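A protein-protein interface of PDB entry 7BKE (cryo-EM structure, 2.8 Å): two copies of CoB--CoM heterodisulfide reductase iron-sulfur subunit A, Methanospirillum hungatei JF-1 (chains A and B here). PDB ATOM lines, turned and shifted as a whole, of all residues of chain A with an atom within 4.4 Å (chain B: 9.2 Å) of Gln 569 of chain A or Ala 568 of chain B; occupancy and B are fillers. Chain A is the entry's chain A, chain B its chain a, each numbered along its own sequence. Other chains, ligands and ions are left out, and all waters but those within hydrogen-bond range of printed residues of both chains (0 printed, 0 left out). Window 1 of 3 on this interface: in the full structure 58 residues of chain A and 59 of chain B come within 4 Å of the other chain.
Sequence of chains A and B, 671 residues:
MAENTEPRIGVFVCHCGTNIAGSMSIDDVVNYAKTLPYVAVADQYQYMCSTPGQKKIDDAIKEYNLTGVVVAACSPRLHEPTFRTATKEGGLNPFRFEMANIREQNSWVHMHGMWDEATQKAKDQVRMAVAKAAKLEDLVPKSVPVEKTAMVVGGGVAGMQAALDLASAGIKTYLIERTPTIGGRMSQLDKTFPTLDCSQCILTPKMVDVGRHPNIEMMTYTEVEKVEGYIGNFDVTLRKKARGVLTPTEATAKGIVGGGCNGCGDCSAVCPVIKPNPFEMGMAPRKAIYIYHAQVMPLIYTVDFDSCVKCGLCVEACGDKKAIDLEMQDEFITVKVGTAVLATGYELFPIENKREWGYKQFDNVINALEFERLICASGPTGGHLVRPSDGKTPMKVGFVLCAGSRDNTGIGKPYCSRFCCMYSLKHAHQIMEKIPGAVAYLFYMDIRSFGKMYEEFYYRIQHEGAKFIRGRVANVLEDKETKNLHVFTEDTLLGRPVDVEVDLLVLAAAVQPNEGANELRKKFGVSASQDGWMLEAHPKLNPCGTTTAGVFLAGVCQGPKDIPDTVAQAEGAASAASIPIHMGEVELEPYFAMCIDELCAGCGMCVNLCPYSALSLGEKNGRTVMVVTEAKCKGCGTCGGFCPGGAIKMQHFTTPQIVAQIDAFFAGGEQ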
ATOM      1  N   PRO A 543      18.756  23.330 -13.386  1.00  0.00           N
ATOM      2  CA  PRO A 543      18.524  22.058 -12.702  1.00  0.00           C
ATOM      3  C   PRO A 543      18.468  22.160 -11.187  1.00  0.00           C
ATOM      4  O   PRO A 543      18.211  21.149 -10.530  1.00  0.00           O
ATOM      5  CB  PRO A 543      19.721  21.214 -13.147  1.00  0.00           C
ATOM      6  CG  PRO A 543      20.797  22.197 -13.376  1.00  0.00           C
ATOM      7  CD  PRO A 543      20.148  23.465 -13.848  1.00  0.00           C
ATOM      8  N   CYS A 544      18.694  23.340 -10.615  1.00  0.00           N
ATOM      9  CA  CYS A 544      18.674  23.513  -9.167  1.00  0.00           C
ATOM     10  C   CYS A 544      17.386  24.148  -8.666  1.00  0.00           C
ATOM     11  O   CYS A 544      16.752  23.626  -7.747  1.00  0.00           O
ATOM     12  CB  CYS A 544      19.875  24.355  -8.728  1.00  0.00           C
ATOM     13  SG  CYS A 544      21.414  23.422  -8.607  1.00  0.00           S
ATOM     14  N   LEU A 553      16.954  22.812  -5.140  1.00  0.00           N
ATOM     15  CA  LEU A 553      17.205  21.388  -5.008  1.00  0.00           C
ATOM     16  C   LEU A 553      18.696  21.105  -5.045  1.00  0.00           C
ATOM     17  O   LEU A 553      19.459  21.797  -5.722  1.00  0.00           O
ATOM     18  CB  LEU A 553      16.519  20.611  -6.129  1.00  0.00           C
ATOM     19  CG  LEU A 553      15.012  20.790  -6.235  1.00  0.00           C
ATOM     20  CD1 LEU A 553      14.488  20.140  -7.490  1.00  0.00           C
ATOM     21  CD2 LEU A 553      14.328  20.235  -5.009  1.00  0.00           C
ATOM     22  N   ALA A 554      19.110  20.076  -4.318  1.00  0.00           N
ATOM     23  CA  ALA A 554      20.509  19.683  -4.307  1.00  0.00           C
ATOM     24  C   ALA A 554      20.616  18.192  -4.037  1.00  0.00           C
ATOM     25  O   ALA A 554      19.949  17.671  -3.142  1.00  0.00           O
ATOM     26  CB  ALA A 554      21.290  20.471  -3.256  1.00  0.00           C
ATOM     27  N   GLY A 555      21.395  17.481  -4.838  1.00  0.00           N
ATOM     28  CA  GLY A 555      21.669  16.074  -4.525  1.00  0.00           C
ATOM     29  C   GLY A 555      20.795  15.052  -5.194  1.00  0.00           C
ATOM     30  O   GLY A 555      20.076  15.388  -6.137  1.00  0.00           O
ATOM     31  N   GLN A 558      16.842  15.224  -6.392  1.00  0.00           N
ATOM     32  CA  GLN A 558      16.399  15.625  -7.717  1.00  0.00           C
ATOM     33  C   GLN A 558      16.612  14.543  -8.769  1.00  0.00           C
ATOM     34  O   GLN A 558      16.164  14.701  -9.907  1.00  0.00           O
ATOM     35  CB  GLN A 558      17.129  16.911  -8.117  1.00  0.00           C
ATOM     36  CG  GLN A 558      16.612  17.598  -9.349  1.00  0.00           C
ATOM     37  CD  GLN A 558      17.539  17.402 -10.522  1.00  0.00           C
ATOM     38  OE1 GLN A 558      18.704  17.054 -10.346  1.00  0.00           O
ATOM     39  NE2 GLN A 558      17.033  17.617 -11.723  1.00  0.00           N
ATOM     40  N   ASP A 565      28.904  14.840  -8.898  1.00  0.00           N
ATOM     41  CA  ASP A 565      27.739  15.522  -9.454  1.00  0.00           C
ATOM     42  C   ASP A 565      26.852  16.079  -8.353  1.00  0.00           C
ATOM     43  O   ASP A 565      26.308  17.181  -8.478  1.00  0.00           O
ATOM     44  CB  ASP A 565      26.940  14.577 -10.345  1.00  0.00           C
ATOM     45  CG  ASP A 565      27.777  13.958 -11.441  1.00  0.00           C
ATOM     46  OD1 ASP A 565      27.263  13.064 -12.145  1.00  0.00           O
ATOM     47  OD2 ASP A 565      28.950  14.361 -11.597  1.00  0.00           O
ATOM     48  N   THR A 566      26.707  15.340  -7.253  1.00  0.00           N
ATOM     49  CA  THR A 566      25.877  15.783  -6.099  1.00  0.00           C
ATOM     50  C   THR A 566      26.482  17.053  -5.502  1.00  0.00           C
ATOM     51  O   THR A 566      25.716  17.959  -5.208  1.00  0.00           O
ATOM     52  CB  THR A 566      25.705  14.664  -5.069  1.00  0.00           C
ATOM     53  OG1 THR A 566      24.723  13.756  -5.559  1.00  0.00           O
ATOM     54  CG2 THR A 566      25.302  15.155  -3.699  1.00  0.00           C
ATOM     55  N   VAL A 567      27.804  17.106  -5.366  1.00  0.00           N
ATOM     56  CA  VAL A 567      28.449  18.265  -4.761  1.00  0.00           C
ATOM     57  C   VAL A 567      28.379  19.468  -5.689  1.00  0.00           C
ATOM     58  O   VAL A 567      28.162  20.602  -5.244  1.00  0.00           O
ATOM     59  CB  VAL A 567      29.896  17.913  -4.375  1.00  0.00           C
ATOM     60  CG1 VAL A 567      30.697  19.158  -4.097  1.00  0.00           C
ATOM     61  CG2 VAL A 567      29.901  17.007  -3.175  1.00  0.00           C
ATOM     62  N   ALA A 568      28.551  19.245  -6.995  1.00  0.00           N
ATOM     63  CA  ALA A 568      28.398  20.336  -7.950  1.00  0.00           C
ATOM     64  C   ALA A 568      26.991  20.909  -7.896  1.00  0.00           C
ATOM     65  O   ALA A 568      26.805  22.133  -7.873  1.00  0.00           O
ATOM     66  CB  ALA A 568      28.729  19.848  -9.356  1.00  0.00           C
ATOM     67  N   GLN A 569      25.985  20.034  -7.846  1.00  0.00           N
ATOM     68  CA  GLN A 569      24.601  20.478  -7.744  1.00  0.00           C
ATOM     69  C   GLN A 569      24.355  21.231  -6.442  1.00  0.00           C
ATOM     70  O   GLN A 569      23.637  22.235  -6.426  1.00  0.00           O
ATOM     71  CB  GLN A 569      23.682  19.263  -7.856  1.00  0.00           C
ATOM     72  CG  GLN A 569      22.210  19.520  -7.649  1.00  0.00           C
ATOM     73  CD  GLN A 569      21.467  19.698  -8.946  1.00  0.00           C
ATOM     74  OE1 GLN A 569      22.066  19.965  -9.984  1.00  0.00           O
ATOM     75  NE2 GLN A 569      20.155  19.522  -8.904  1.00  0.00           N
ATOM     76  N   ALA A 570      24.934  20.754  -5.340  1.00  0.00           N
ATOM     77  CA  ALA A 570      24.752  21.401  -4.045  1.00  0.00           C
ATOM     78  C   ALA A 570      25.346  22.804  -4.030  1.00  0.00           C
ATOM     79  O   ALA A 570      24.726  23.738  -3.509  1.00  0.00           O
ATOM     80  CB  ALA A 570      25.369  20.547  -2.940  1.00  0.00           C
ATOM     81  N   GLU A 571      26.539  22.981  -4.608  1.00  0.00           N
ATOM     82  CA  GLU A 571      27.118  24.321  -4.640  1.00  0.00           C
ATOM     83  C   GLU A 571      26.348  25.225  -5.588  1.00  0.00           C
ATOM     84  O   GLU A 571      26.204  26.425  -5.327  1.00  0.00           O
ATOM     85  CB  GLU A 571      28.591  24.293  -5.034  1.00  0.00           C
ATOM     86  CG  GLU A 571      29.521  23.867  -3.921  1.00  0.00           C
ATOM     87  CD  GLU A 571      30.839  23.398  -4.463  1.00  0.00           C
ATOM     88  OE1 GLU A 571      30.940  22.223  -4.871  1.00  0.00           O
ATOM     89  OE2 GLU A 571      31.795  24.205  -4.450  1.00  0.00           O
ATOM     90  N   GLY A 572      25.847  24.674  -6.693  1.00  0.00           N
ATOM     91  CA  GLY A 572      24.994  25.458  -7.566  1.00  0.00           C
ATOM     92  C   GLY A 572      23.748  25.946  -6.855  1.00  0.00           C
ATOM     93  O   GLY A 572      23.352  27.106  -6.994  1.00  0.00           O
ATOM     94  N   ALA A 573      23.124  25.070  -6.067  1.00  0.00           N
ATOM     95  CA  ALA A 573      21.944  25.462  -5.307  1.00  0.00           C
ATOM     96  C   ALA A 573      22.286  26.506  -4.255  1.00  0.00           C
ATOM     97  O   ALA A 573      21.506  27.430  -4.019  1.00  0.00           O
ATOM     98  CB  ALA A 573      21.307  24.237  -4.659  1.00  0.00           C
ATOM     99  N   VAL B 157      27.850  27.892 -22.691  1.00  0.00           N
ATOM    100  CA  VAL B 157      26.800  27.876 -21.639  1.00  0.00           C
ATOM    101  C   VAL B 157      27.437  27.949 -20.249  1.00  0.00           C
ATOM    102  O   VAL B 157      26.871  28.614 -19.393  1.00  0.00           O
ATOM    103  CB  VAL B 157      25.822  26.699 -21.816  1.00  0.00           C
ATOM    104  CG1 VAL B 157      26.434  25.340 -21.520  1.00  0.00           C
ATOM    105  CG2 VAL B 157      24.530  26.901 -21.047  1.00  0.00           C
ATOM    106  N   ALA B 158      28.538  27.239 -20.018  1.00  0.00           N
ATOM    107  CA  ALA B 158      29.176  27.227 -18.685  1.00  0.00           C
ATOM    108  C   ALA B 158      29.783  28.577 -18.334  1.00  0.00           C
ATOM    109  O   ALA B 158      29.678  28.983 -17.203  1.00  0.00           O
ATOM    110  CB  ALA B 158      30.239  26.183 -18.658  1.00  0.00           C
ATOM    111  N   GLN B 161      26.725  31.010 -17.794  1.00  0.00           N
ATOM    112  CA  GLN B 161      26.068  30.760 -16.519  1.00  0.00           C
ATOM    113  C   GLN B 161      26.908  31.259 -15.352  1.00  0.00           C
ATOM    114  O   GLN B 161      26.382  31.871 -14.419  1.00  0.00           O
ATOM    115  CB  GLN B 161      25.779  29.274 -16.370  1.00  0.00           C
ATOM    116  CG  GLN B 161      24.872  28.942 -15.213  1.00  0.00           C
ATOM    117  CD  GLN B 161      23.678  29.871 -15.114  1.00  0.00           C
ATOM    118  OE1 GLN B 161      22.704  29.726 -15.847  1.00  0.00           O
ATOM    119  NE2 GLN B 161      23.738  30.817 -14.189  1.00  0.00           N
ATOM    120  N   ALA B 162      28.218  31.007 -15.387  1.00  0.00           N
ATOM    121  CA  ALA B 162      29.087  31.487 -14.319  1.00  0.00           C
ATOM    122  C   ALA B 162      29.106  33.012 -14.262  1.00  0.00           C
ATOM    123  O   ALA B 162      29.055  33.600 -13.177  1.00  0.00           O
ATOM    124  CB  ALA B 162      30.494  30.937 -14.510  1.00  0.00           C
ATOM    125  N   ASP B 165      25.792  34.265 -12.872  1.00  0.00           N
ATOM    126  CA  ASP B 165      25.716  33.980 -11.446  1.00  0.00           C
ATOM    127  C   ASP B 165      26.546  34.969 -10.635  1.00  0.00           C
ATOM    128  O   ASP B 165      26.072  35.520  -9.637  1.00  0.00           O
ATOM    129  CB  ASP B 165      26.174  32.549 -11.189  1.00  0.00           C
ATOM    130  CG  ASP B 165      25.762  32.046  -9.835  1.00  0.00           C
ATOM    131  OD1 ASP B 165      26.335  32.517  -8.829  1.00  0.00           O
ATOM    132  OD2 ASP B 165      24.869  31.176  -9.767  1.00  0.00           O
ATOM    133  N   LYS B 452      18.600  11.778 -16.149  1.00  0.00           N
ATOM    134  CA  LYS B 452      17.179  11.905 -15.852  1.00  0.00           C
ATOM    135  C   LYS B 452      16.377  11.917 -17.144  1.00  0.00           C
ATOM    136  O   LYS B 452      16.618  12.752 -18.020  1.00  0.00           O
ATOM    137  CB  LYS B 452      16.928  13.172 -15.045  1.00  0.00           C
ATOM    138  CG  LYS B 452      15.622  13.169 -14.288  1.00  0.00           C
ATOM    139  CD  LYS B 452      15.462  14.420 -13.461  1.00  0.00           C
ATOM    140  CE  LYS B 452      14.193  14.357 -12.642  1.00  0.00           C
ATOM    141  NZ  LYS B 452      14.226  15.311 -11.509  1.00  0.00           N
ATOM    142  N   PRO B 543      35.011  19.203  -7.233  1.00  0.00           N
ATOM    143  CA  PRO B 543      35.176  19.069  -8.682  1.00  0.00           C
ATOM    144  C   PRO B 543      35.301  20.387  -9.425  1.00  0.00           C
ATOM    145  O   PRO B 543      35.509  20.369 -10.641  1.00  0.00           O
ATOM    146  CB  PRO B 543      33.902  18.327  -9.095  1.00  0.00           C
ATOM    147  CG  PRO B 543      32.894  18.749  -8.106  1.00  0.00           C
ATOM    148  CD  PRO B 543      33.616  18.995  -6.813  1.00  0.00           C
ATOM    149  N   CYS B 544      35.186  21.523  -8.742  1.00  0.00           N
ATOM    150  CA  CYS B 544      35.277  22.827  -9.389  1.00  0.00           C
ATOM    151  C   CYS B 544      36.629  23.494  -9.182  1.00  0.00           C
ATOM    152  O   CYS B 544      37.258  23.933 -10.147  1.00  0.00           O
ATOM    153  CB  CYS B 544      34.161  23.740  -8.878  1.00  0.00           C
ATOM    154  SG  CYS B 544      32.563  23.451  -9.662  1.00  0.00           S
ATOM    155  N   LEU B 553      37.103  25.688 -12.244  1.00  0.00           N
ATOM    156  CA  LEU B 553      36.753  25.043 -13.498  1.00  0.00           C
ATOM    157  C   LEU B 553      35.245  24.970 -13.654  1.00  0.00           C
ATOM    158  O   LEU B 553      34.509  24.836 -12.676  1.00  0.00           O
ATOM    159  CB  LEU B 553      37.333  23.633 -13.563  1.00  0.00           C
ATOM    160  CG  LEU B 553      38.844  23.529 -13.415  1.00  0.00           C
ATOM    161  CD1 LEU B 553      39.267  22.088 -13.295  1.00  0.00           C
ATOM    162  CD2 LEU B 553      39.534  24.203 -14.577  1.00  0.00           C
ATOM    163  N   ALA B 554      34.785  25.050 -14.896  1.00  0.00           N
ATOM    164  CA  ALA B 554      33.363  24.950 -15.175  1.00  0.00           C
ATOM    165  C   ALA B 554      33.156  24.374 -16.567  1.00  0.00           C
ATOM    166  O   ALA B 554      33.820  24.791 -17.517  1.00  0.00           O
ATOM    167  CB  ALA B 554      32.685  26.316 -15.058  1.00  0.00           C
ATOM    168  N   GLY B 555      32.296  23.377 -16.692  1.00  0.00           N
ATOM    169  CA  GLY B 555      31.932  22.895 -18.030  1.00  0.00           C
ATOM    170  C   GLY B 555      32.699  21.715 -18.554  1.00  0.00           C
ATOM    171  O   GLY B 555      33.402  21.057 -17.787  1.00  0.00           O
ATOM    172  N   LYS B 561      30.401  16.465 -20.509  1.00  0.00           N
ATOM    173  CA  LYS B 561      29.150  16.475 -19.708  1.00  0.00           C
ATOM    174  C   LYS B 561      28.005  17.019 -20.545  1.00  0.00           C
ATOM    175  O   LYS B 561      28.280  17.687 -21.517  1.00  0.00           O
ATOM    176  CB  LYS B 561      29.310  17.437 -18.536  1.00  0.00           C
ATOM    177  CG  LYS B 561      29.717  16.841 -17.199  1.00  0.00           C
ATOM    178  CD  LYS B 561      30.260  17.899 -16.269  1.00  0.00           C
ATOM    179  CE  LYS B 561      31.701  17.665 -15.879  1.00  0.00           C
ATOM    180  NZ  LYS B 561      32.605  18.634 -16.539  1.00  0.00           N
ATOM    181  N   ASP B 562      26.764  16.750 -20.158  1.00  0.00           N
ATOM    182  CA  ASP B 562      25.573  17.312 -20.836  1.00  0.00           C
ATOM    183  C   ASP B 562      25.339  18.742 -20.345  1.00  0.00           C
ATOM    184  O   ASP B 562      25.976  19.130 -19.385  1.00  0.00           O
ATOM    185  CB  ASP B 562      24.354  16.421 -20.621  1.00  0.00           C
ATOM    186  CG  ASP B 562      24.262  15.847 -19.225  1.00  0.00           C
ATOM    187  OD1 ASP B 562      24.951  14.841 -18.962  1.00  0.00           O
ATOM    188  OD2 ASP B 562      23.501  16.403 -18.419  1.00  0.00           O
ATOM    189  N   ILE B 563      24.462  19.495 -21.003  1.00  0.00           N
ATOM    190  CA  ILE B 563      24.188  20.918 -20.656  1.00  0.00           C
ATOM    191  C   ILE B 563      23.688  21.042 -19.216  1.00  0.00           C
ATOM    192  O   ILE B 563      24.156  21.947 -18.550  1.00  0.00           O
ATOM    193  CB  ILE B 563      23.256  21.568 -21.692  1.00  0.00           C
ATOM    194  CG1 ILE B 563      23.926  21.674 -23.064  1.00  0.00           C
ATOM    195  CG2 ILE B 563      22.742  22.913 -21.210  1.00  0.00           C
ATOM    196  CD1 ILE B 563      22.953  21.795 -24.206  1.00  0.00           C
ATOM    197  N   PRO B 564      22.800  20.176 -18.676  1.00  0.00           N
ATOM    198  CA  PRO B 564      22.429  20.220 -17.250  1.00  0.00           C
ATOM    199  C   PRO B 564      23.594  20.120 -16.256  1.00  0.00           C
ATOM    200  O   PRO B 564      23.653  20.928 -15.384  1.00  0.00           O
ATOM    201  CB  PRO B 564      21.577  18.959 -17.122  1.00  0.00           C
ATOM    202  CG  PRO B 564      20.881  18.862 -18.433  1.00  0.00           C
ATOM    203  CD  PRO B 564      21.983  19.199 -19.403  1.00  0.00           C
ATOM    204  N   ASP B 565      24.454  19.107 -16.382  1.00  0.00           N
ATOM    205  CA  ASP B 565      25.641  18.924 -15.556  1.00  0.00           C
ATOM    206  C   ASP B 565      26.611  20.082 -15.726  1.00  0.00           C
ATOM    207  O   ASP B 565      27.231  20.534 -14.758  1.00  0.00           O
ATOM    208  CB  ASP B 565      26.331  17.606 -15.892  1.00  0.00           C
ATOM    209  CG  ASP B 565      25.407  16.417 -15.777  1.00  0.00           C
ATOM    210  OD1 ASP B 565      25.825  15.303 -16.161  1.00  0.00           O
ATOM    211  OD2 ASP B 565      24.262  16.592 -15.308  1.00  0.00           O
ATOM    212  N   THR B 566      26.746  20.590 -16.951  1.00  0.00           N
ATOM    213  CA  THR B 566      27.653  21.735 -17.244  1.00  0.00           C
ATOM    214  C   THR B 566      27.167  22.968 -16.484  1.00  0.00           C
ATOM    215  O   THR B 566      28.010  23.649 -15.918  1.00  0.00           O
ATOM    216  CB  THR B 566      27.783  21.977 -18.750  1.00  0.00           C
ATOM    217  OG1 THR B 566      28.674  21.000 -19.282  1.00  0.00           O
ATOM    218  CG2 THR B 566      28.277  23.357 -19.103  1.00  0.00           C
ATOM    219  N   VAL B 567      25.860  23.208 -16.460  1.00  0.00           N
ATOM    220  CA  VAL B 567      25.328  24.392 -15.796  1.00  0.00           C
ATOM    221  C   VAL B 567      25.449  24.264 -14.286  1.00  0.00           C
ATOM    222  O   VAL B 567      25.767  25.236 -13.588  1.00  0.00           O
ATOM    223  CB  VAL B 567      23.877  24.631 -16.243  1.00  0.00           C
ATOM    224  CG1 VAL B 567      23.181  25.599 -15.321  1.00  0.00           C
ATOM    225  CG2 VAL B 567      23.853  25.144 -17.656  1.00  0.00           C
ATOM    226  N   ALA B 568      25.209  23.063 -13.752  1.00  0.00           N
ATOM    227  CA  ALA B 568      25.403  22.846 -12.324  1.00  0.00           C
ATOM    228  C   ALA B 568      26.850  23.097 -11.929  1.00  0.00           C
ATOM    229  O   ALA B 568      27.127  23.765 -10.924  1.00  0.00           O
ATOM    230  CB  ALA B 568      24.980  21.428 -11.951  1.00  0.00           C
ATOM    231  N   GLN B 569      27.789  22.588 -12.728  1.00  0.00           N
ATOM    232  CA  GLN B 569      29.204  22.811 -12.469  1.00  0.00           C
ATOM    233  C   GLN B 569      29.560  24.290 -12.560  1.00  0.00           C
ATOM    234  O   GLN B 569      30.350  24.795 -11.758  1.00  0.00           O
ATOM    235  CB  GLN B 569      30.025  21.990 -13.461  1.00  0.00           C
ATOM    236  CG  GLN B 569      31.521  22.193 -13.418  1.00  0.00           C
ATOM    237  CD  GLN B 569      32.220  21.149 -12.589  1.00  0.00           C
ATOM    238  OE1 GLN B 569      31.602  20.470 -11.775  1.00  0.00           O
ATOM    239  NE2 GLN B 569      33.517  20.992 -12.812  1.00  0.00           N
ATOM    240  N   ALA B 570      28.991  24.997 -13.539  1.00  0.00           N
ATOM    241  CA  ALA B 570      29.273  26.418 -13.712  1.00  0.00           C
ATOM    242  C   ALA B 570      28.785  27.237 -12.521  1.00  0.00           C
ATOM    243  O   ALA B 570      29.493  28.132 -12.050  1.00  0.00           O
ATOM    244  CB  ALA B 570      28.640  26.925 -15.004  1.00  0.00           C
ATOM    245  N   GLU B 571      27.587  26.938 -12.010  1.00  0.00           N
ATOM    246  CA  GLU B 571      27.108  27.681 -10.848  1.00  0.00           C
ATOM    247  C   GLU B 571      27.903  27.321  -9.605  1.00  0.00           C
ATOM    248  O   GLU B 571      28.145  28.180  -8.751  1.00  0.00           O
ATOM    249  CB  GLU B 571      25.622  27.446 -10.599  1.00  0.00           C
ATOM    250  CG  GLU B 571      24.709  28.215 -11.525  1.00  0.00           C
ATOM    251  CD  GLU B 571      23.339  27.604 -11.569  1.00  0.00           C
ATOM    252  OE1 GLU B 571      23.134  26.634 -12.326  1.00  0.00           O
ATOM    253  OE2 GLU B 571      22.446  28.125 -10.863  1.00  0.00           O
ATOM    254  N   GLY B 572      28.317  26.060  -9.482  1.00  0.00           N
ATOM    255  CA  GLY B 572      29.190  25.692  -8.384  1.00  0.00           C
ATOM    256  C   GLY B 572      30.496  26.460  -8.413  1.00  0.00           C
ATOM    257  O   GLY B 572      30.971  26.943  -7.383  1.00  0.00           O
ATOM    258  N   ALA B 573      31.085  26.596  -9.602  1.00  0.00           N
ATOM    259  CA  ALA B 573      32.320  27.356  -9.737  1.00  0.00           C
ATOM    260  C   ALA B 573      32.099  28.830  -9.425  1.00  0.00           C
ATOM    261  O   ALA B 573      32.955  29.471  -8.812  1.00  0.00           O
ATOM    262  CB  ALA B 573      32.890  27.187 -11.140  1.00  0.00           C
ATOM    263  N   ALA B 574      30.967  29.388  -9.854  1.00  0.00           N
ATOM    264  CA  ALA B 574      30.674  30.781  -9.534  1.00  0.00           C
ATOM    265  C   ALA B 574      30.551  30.984  -8.031  1.00  0.00           C
ATOM    266  O   ALA B 574      31.040  31.979  -7.489  1.00  0.00           O
ATOM    267  CB  ALA B 574      29.401  31.233 -10.241  1.00  0.00           C
ATOM    268  N   SER B 575      29.910  30.044  -7.336  1.00  0.00           N
ATOM    269  CA  SER B 575      29.818  30.139  -5.884  1.00  0.00           C
ATOM    270  C   SER B 575      31.198  30.081  -5.238  1.00  0.00           C
ATOM    271  O   SER B 575      31.508  30.858  -4.323  1.00  0.00           O
ATOM    272  CB  SER B 575      28.935  29.017  -5.344  1.00  0.00           C
ATOM    273  OG  SER B 575      28.699  29.201  -3.968  1.00  0.00           O
ATOM    274  N   ALA B 576      32.042  29.155  -5.699  1.00  0.00           N
ATOM    275  CA  ALA B 576      33.376  29.031  -5.120  1.00  0.00           C
ATOM    276  C   ALA B 576      34.209  30.281  -5.385  1.00  0.00           C
ATOM    277  O   ALA B 576      34.996  30.699  -4.533  1.00  0.00           O
ATOM    278  CB  ALA B 576      34.073  27.787  -5.658  1.00  0.00           C
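The backbone carbonyl oxygen (O) of Gln 558 of chain A is in hydrogen-bond range of the side-chain amino group (NZ) of Lys 452 of chain B.
The backbone carbonyl oxygen of Ala 568 of chain A sits close to the backbone carbonyl oxygen of Ala 568 of chain B (3.5 Å).
NE2 of Gln 569 of chain A sits at hydrogen-bond distance from O of Pro 543 of chain A.
O of Gln 569 of chain A sits at hydrogen-bond distance from SG of Cys 544 of chain A, at 3.3 Å.
OE1 of Gln 558 of chain A is in hydrogen-bond range of NE2 of Gln 569 of chain A (3.2 Å).
The backbone carbonyl oxygen of Pro 543 of chain B sits at hydrogen-bond distance from the side-chain amide nitrogen of Gln 569 of chain B (3.0 Å).
SG of Cys 544 of chain B is in hydrogen-bond range of O of Gln 569 of chain B (3.3 Å).
Among the printed residues, pairs that only touch across the chains: Pro 543 of chain A with Pro 564 of chain B (3.7 Å), Pro 543 of chain A with Val 567 of chain B (3.99 Å), Val 567 of chain A with Pro 543 of chain B (3.99 Å), Ala 568 of chain A with Gln 569 of chain B (3.8 Å), Gln 569 of chain A with Ala 568 of chain B (3.8 Å), Glu 571 of chain A with Gly 572 of chain B (3.7 Å), Glu 571 of chain A with Ser 575 of chain B (3.8 Å), Gly 572 of chain A with Glu 571 of chain B (3.7 Å) and Gly 572 of chain A with Gly 572 of chain B (3.9 Å).
Of the printed residues of chain B, Gln 569 of chain A touches Ala 568 (3.8 Å).
Ala 568 of chain B touches just these residues of chain A: Ala 568 (3.5 Å) and Gln 569 (3.8 Å).
Of chain B, only Ala 568 (3.5 Å) and Gln 569 (3.8 Å) come within 4 Å of Ala 568 of chain A.
Printed residues of chain B within 4 Å of Gly 572 of chain A: Glu 571 (3.7 Å) and Gly 572 (3.9 Å).
Printed residues of chain A within 4 Å of Glu 571 of chain B: Gly 572 (3.7 Å).
Of the printed residues of chain A, Ser 575 of chain B touches Glu 571.
Of the printed residues of chain A, Gln 569 of chain B touches Ala 568 (3.8 Å).
Printed residues of chain B within 4 Å of Glu 571 of chain A: Gly 572 (3.7 Å) and Ser 575 (3.8 Å).
Ala 554 of chain A touches none of the printed residues of chain B.
Cys 544 of chain A touches none of the printed residues of chain B.
The nearest residue of chain B that does not touch Gln 569 of chain A is Pro 564 of chain B (5.7 Å).
Of the 27 printed residues of chain B, 9 touch a printed residue of chain A.
Hydrophobic or aromatic side chains of chain B that line the printed part of chain A: Pro 543, Val 567 and Ala 568.
Among the printed residues, no Asp or Glu carboxylate lies within 4 Å of a Lys or Arg side-chain nitrogen of the other chain.
Pro 543 of chain A touches Val 567 of chain B, and with the chains exchanged Val 567 of chain A touches Pro 543 of chain B.
Ala 568 of chain B touches its own counterpart, Ala 568 of chain A.
Ala 568 of chain A touches Gln 569 of chain B, and with the chains exchanged Gln 569 of chain A touches Ala 568 of chain B.
Gly 572 of chain A touches its own counterpart, Gly 572 of chain B.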
